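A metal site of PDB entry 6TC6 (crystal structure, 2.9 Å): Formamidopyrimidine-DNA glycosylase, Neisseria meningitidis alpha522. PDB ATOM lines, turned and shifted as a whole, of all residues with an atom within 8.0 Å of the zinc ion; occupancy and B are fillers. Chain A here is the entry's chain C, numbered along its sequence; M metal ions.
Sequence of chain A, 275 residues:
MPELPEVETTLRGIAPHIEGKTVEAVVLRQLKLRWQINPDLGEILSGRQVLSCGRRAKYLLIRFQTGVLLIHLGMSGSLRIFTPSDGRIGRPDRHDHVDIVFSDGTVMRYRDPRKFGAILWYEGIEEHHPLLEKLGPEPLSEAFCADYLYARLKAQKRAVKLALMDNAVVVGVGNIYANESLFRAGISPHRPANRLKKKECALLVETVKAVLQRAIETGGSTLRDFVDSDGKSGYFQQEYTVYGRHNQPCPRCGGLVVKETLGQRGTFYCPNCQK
The zinc ion is bound by the side-chain sulfur of Cys 273 (2.3 Å), the side-chain sulfur of Cys 253 (2.3 Å) and the side-chain sulfur of Cys 270 (2.3 Å).
Slightly farther from the zinc ion lies SG of Cys 250 (2.9 Å).
Four residues have an atom within 4 Å of the zinc ion: Cys 250, Cys 253, Cys 270 and Cys 273.
The nearest printed residue that does not touch the zinc ion is Gly 254 (4.3 Å).
NE of Arg 252 lies close to SG of Cys 273.
The side-chain sulfur (SG) of Cys 250 is in hydrogen-bond range of the backbone NH (N) of Cys 253.
N of Gly 255 sits close to SG of Cys 253 (2.5 Å).
The side-chain sulfur of Cys 270 lies close to the backbone NH of Asn 272, 3.4 Å away.
The side-chain amide oxygen (OE1) of Gln 274 is in hydrogen-bond range of the backbone NH (N) of Cys 270, 3.3 Å away.
The backbone carbonyl oxygen (O) of Gly 255 sits at hydrogen-bond distance from the backbone NH (N) of Cys 250 (3.0 Å).
SG of Cys 250 sits close to N of Arg 252, at 3.3 Å.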
ATOM      1  N   PHE A 183     -11.176  -5.280  -7.779  1.00  0.00           N
ATOM      2  CA  PHE A 183     -12.267  -6.247  -7.747  1.00  0.00           C
ATOM      3  C   PHE A 183     -12.296  -7.005  -6.431  1.00  0.00           C
ATOM      4  O   PHE A 183     -13.325  -7.072  -5.756  1.00  0.00           O
ATOM      5  CB  PHE A 183     -12.180  -7.221  -8.915  1.00  0.00           C
ATOM      6  CG  PHE A 183     -13.026  -8.452  -8.725  1.00  0.00           C
ATOM      7  CD1 PHE A 183     -14.404  -8.393  -8.880  1.00  0.00           C
ATOM      8  CD2 PHE A 183     -12.453  -9.663  -8.351  1.00  0.00           C
ATOM      9  CE1 PHE A 183     -15.187  -9.515  -8.695  1.00  0.00           C
ATOM     10  CE2 PHE A 183     -13.236 -10.785  -8.166  1.00  0.00           C
ATOM     11  CZ  PHE A 183     -14.601 -10.714  -8.334  1.00  0.00           C
ATOM     12  N   PRO A 249     -18.804 -14.533 -16.732  1.00  0.00           N
ATOM     13  CA  PRO A 249     -19.508 -14.364 -15.451  1.00  0.00           C
ATOM     14  C   PRO A 249     -18.548 -14.159 -14.284  1.00  0.00           C
ATOM     15  O   PRO A 249     -17.411 -14.641 -14.277  1.00  0.00           O
ATOM     16  CB  PRO A 249     -20.281 -15.681 -15.297  1.00  0.00           C
ATOM     17  CG  PRO A 249     -19.603 -16.646 -16.219  1.00  0.00           C
ATOM     18  CD  PRO A 249     -19.108 -15.827 -17.368  1.00  0.00           C
ATOM     19  N   CYS A 250     -19.021 -13.404 -13.293  1.00  0.00           N
ATOM     20  CA  CYS A 250     -18.191 -13.036 -12.166  1.00  0.00           C
ATOM     21  C   CYS A 250     -18.082 -14.204 -11.193  1.00  0.00           C
ATOM     22  O   CYS A 250     -19.055 -14.944 -10.993  1.00  0.00           O
ATOM     23  CB  CYS A 250     -18.773 -11.815 -11.451  1.00  0.00           C
ATOM     24  SG  CYS A 250     -18.113 -11.498  -9.792  1.00  0.00           S
ATOM     25  N   PRO A 251     -16.922 -14.404 -10.567  1.00  0.00           N
ATOM     26  CA  PRO A 251     -16.762 -15.545  -9.647  1.00  0.00           C
ATOM     27  C   PRO A 251     -17.586 -15.419  -8.376  1.00  0.00           C
ATOM     28  O   PRO A 251     -17.869 -16.449  -7.749  1.00  0.00           O
ATOM     29  CB  PRO A 251     -15.257 -15.539  -9.348  1.00  0.00           C
ATOM     30  CG  PRO A 251     -14.634 -14.800 -10.494  1.00  0.00           C
ATOM     31  CD  PRO A 251     -15.635 -13.752 -10.870  1.00  0.00           C
ATOM     32  N   ARG A 252     -17.973 -14.212  -7.980  1.00  0.00           N
ATOM     33  CA  ARG A 252     -18.664 -14.023  -6.705  1.00  0.00           C
ATOM     34  C   ARG A 252     -20.180 -13.898  -6.880  1.00  0.00           C
ATOM     35  O   ARG A 252     -20.911 -14.868  -6.675  1.00  0.00           O
ATOM     36  CB  ARG A 252     -18.112 -12.806  -5.962  1.00  0.00           C
ATOM     37  CG  ARG A 252     -18.720 -12.608  -4.581  1.00  0.00           C
ATOM     38  CD  ARG A 252     -18.162 -11.390  -3.854  1.00  0.00           C
ATOM     39  NE  ARG A 252     -17.642 -10.367  -4.766  1.00  0.00           N
ATOM     40  CZ  ARG A 252     -16.398  -9.911  -4.744  1.00  0.00           C
ATOM     41  NH1 ARG A 252     -15.524 -10.389  -3.865  1.00  0.00           N
ATOM     42  NH2 ARG A 252     -16.016  -8.980  -5.609  1.00  0.00           N
ATOM     43  N   CYS A 253     -20.654 -12.693  -7.237  1.00  0.00           N
ATOM     44  CA  CYS A 253     -22.045 -12.521  -7.646  1.00  0.00           C
ATOM     45  C   CYS A 253     -22.416 -13.481  -8.770  1.00  0.00           C
ATOM     46  O   CYS A 253     -23.375 -14.261  -8.661  1.00  0.00           O
ATOM     47  CB  CYS A 253     -22.306 -11.081  -8.077  1.00  0.00           C
ATOM     48  SG  CYS A 253     -21.894 -10.732  -9.789  1.00  0.00           S
ATOM     49  N   GLY A 254     -21.671 -13.427  -9.881  1.00  0.00           N
ATOM     50  CA  GLY A 254     -22.040 -14.066 -11.124  1.00  0.00           C
ATOM     51  C   GLY A 254     -22.448 -13.137 -12.245  1.00  0.00           C
ATOM     52  O   GLY A 254     -22.869 -13.613 -13.301  1.00  0.00           O
ATOM     53  N   GLY A 255     -22.356 -11.815 -12.047  1.00  0.00           N
ATOM     54  CA  GLY A 255     -22.875 -10.854 -12.996  1.00  0.00           C
ATOM     55  C   GLY A 255     -21.960 -10.680 -14.196  1.00  0.00           C
ATOM     56  O   GLY A 255     -20.846 -11.196 -14.281  1.00  0.00           O
ATOM     57  N   LEU A 256     -22.458  -9.906 -15.166  1.00  0.00           N
ATOM     58  CA  LEU A 256     -21.643  -9.460 -16.291  1.00  0.00           C
ATOM     59  C   LEU A 256     -20.594  -8.476 -15.795  1.00  0.00           C
ATOM     60  O   LEU A 256     -20.927  -7.366 -15.364  1.00  0.00           O
ATOM     61  CB  LEU A 256     -22.525  -8.805 -17.355  1.00  0.00           C
ATOM     62  CG  LEU A 256     -21.778  -8.036 -18.460  1.00  0.00           C
ATOM     63  CD1 LEU A 256     -20.665  -8.865 -19.089  1.00  0.00           C
ATOM     64  CD2 LEU A 256     -22.719  -7.488 -19.535  1.00  0.00           C
ATOM     65  N   VAL A 257     -19.327  -8.864 -15.856  1.00  0.00           N
ATOM     66  CA  VAL A 257     -18.222  -7.951 -15.580  1.00  0.00           C
ATOM     67  C   VAL A 257     -17.840  -7.269 -16.892  1.00  0.00           C
ATOM     68  O   VAL A 257     -17.824  -7.893 -17.963  1.00  0.00           O
ATOM     69  CB  VAL A 257     -17.024  -8.680 -14.938  1.00  0.00           C
ATOM     70  CG1 VAL A 257     -17.484  -9.512 -13.766  1.00  0.00           C
ATOM     71  CG2 VAL A 257     -16.307  -9.564 -15.950  1.00  0.00           C
ATOM     72  N   TYR A 269     -14.272  -4.723 -14.361  1.00  0.00           N
ATOM     73  CA  TYR A 269     -14.869  -4.759 -13.028  1.00  0.00           C
ATOM     74  C   TYR A 269     -16.310  -5.240 -13.099  1.00  0.00           C
ATOM     75  O   TYR A 269     -16.968  -5.167 -14.132  1.00  0.00           O
ATOM     76  CB  TYR A 269     -14.792  -3.387 -12.351  1.00  0.00           C
ATOM     77  CG  TYR A 269     -15.908  -2.449 -12.748  1.00  0.00           C
ATOM     78  CD1 TYR A 269     -17.014  -2.266 -11.919  1.00  0.00           C
ATOM     79  CD2 TYR A 269     -15.860  -1.751 -13.939  1.00  0.00           C
ATOM     80  CE1 TYR A 269     -18.038  -1.407 -12.277  1.00  0.00           C
ATOM     81  CE2 TYR A 269     -16.875  -0.888 -14.300  1.00  0.00           C
ATOM     82  CZ  TYR A 269     -17.960  -0.726 -13.471  1.00  0.00           C
ATOM     83  OH  TYR A 269     -18.966   0.141 -13.835  1.00  0.00           O
ATOM     84  N   CYS A 270     -16.793  -5.724 -11.942  1.00  0.00           N
ATOM     85  CA  CYS A 270     -18.161  -6.224 -11.797  1.00  0.00           C
ATOM     86  C   CYS A 270     -19.094  -5.148 -11.296  1.00  0.00           C
ATOM     87  O   CYS A 270     -19.054  -4.816 -10.095  1.00  0.00           O
ATOM     88  CB  CYS A 270     -18.200  -7.418 -10.862  1.00  0.00           C
ATOM     89  SG  CYS A 270     -19.883  -8.021 -10.556  1.00  0.00           S
ATOM     90  N   PRO A 271     -19.977  -4.591 -12.129  1.00  0.00           N
ATOM     91  CA  PRO A 271     -20.894  -3.542 -11.656  1.00  0.00           C
ATOM     92  C   PRO A 271     -21.860  -3.999 -10.554  1.00  0.00           C
ATOM     93  O   PRO A 271     -22.498  -3.141  -9.922  1.00  0.00           O
ATOM     94  CB  PRO A 271     -21.674  -3.154 -12.927  1.00  0.00           C
ATOM     95  CG  PRO A 271     -20.830  -3.644 -14.069  1.00  0.00           C
ATOM     96  CD  PRO A 271     -20.123  -4.868 -13.568  1.00  0.00           C
ATOM     97  N   ASN A 272     -21.988  -5.301 -10.307  1.00  0.00           N
ATOM     98  CA  ASN A 272     -22.889  -5.795  -9.271  1.00  0.00           C
ATOM     99  C   ASN A 272     -22.210  -5.981  -7.920  1.00  0.00           C
ATOM    100  O   ASN A 272     -22.905  -6.082  -6.899  1.00  0.00           O
ATOM    101  CB  ASN A 272     -23.511  -7.128  -9.699  1.00  0.00           C
ATOM    102  CG  ASN A 272     -24.345  -6.993 -10.963  1.00  0.00           C
ATOM    103  OD1 ASN A 272     -24.356  -5.947 -11.603  1.00  0.00           O
ATOM    104  ND2 ASN A 272     -25.053  -8.054 -11.312  1.00  0.00           N
ATOM    105  N   CYS A 273     -20.872  -6.029  -7.883  1.00  0.00           N
ATOM    106  CA  CYS A 273     -20.100  -6.237  -6.673  1.00  0.00           C
ATOM    107  C   CYS A 273     -19.689  -4.928  -5.997  1.00  0.00           C
ATOM    108  O   CYS A 273     -19.945  -4.728  -4.803  1.00  0.00           O
ATOM    109  CB  CYS A 273     -18.838  -7.055  -6.976  1.00  0.00           C
ATOM    110  SG  CYS A 273     -19.034  -8.843  -6.999  1.00  0.00           S
ATOM    111  N   GLN A 274     -19.067  -4.040  -6.766  1.00  0.00           N
ATOM    112  CA  GLN A 274     -18.059  -3.124  -6.279  1.00  0.00           C
ATOM    113  C   GLN A 274     -18.609  -1.848  -5.640  1.00  0.00           C
ATOM    114  O   GLN A 274     -17.810  -0.992  -5.258  1.00  0.00           O
ATOM    115  CB  GLN A 274     -17.116  -2.776  -7.428  1.00  0.00           C
ATOM    116  CG  GLN A 274     -16.810  -3.976  -8.315  1.00  0.00           C
ATOM    117  CD  GLN A 274     -15.340  -4.273  -8.437  1.00  0.00           C
ATOM    118  OE1 GLN A 274     -14.908  -4.924  -9.372  1.00  0.00           O
ATOM    119  NE2 GLN A 274     -14.556  -3.768  -7.486  1.00  0.00           N
HETATM  120 ZN    ZN M   1     -20.071  -9.614  -8.853  1.00  0.00          ZN
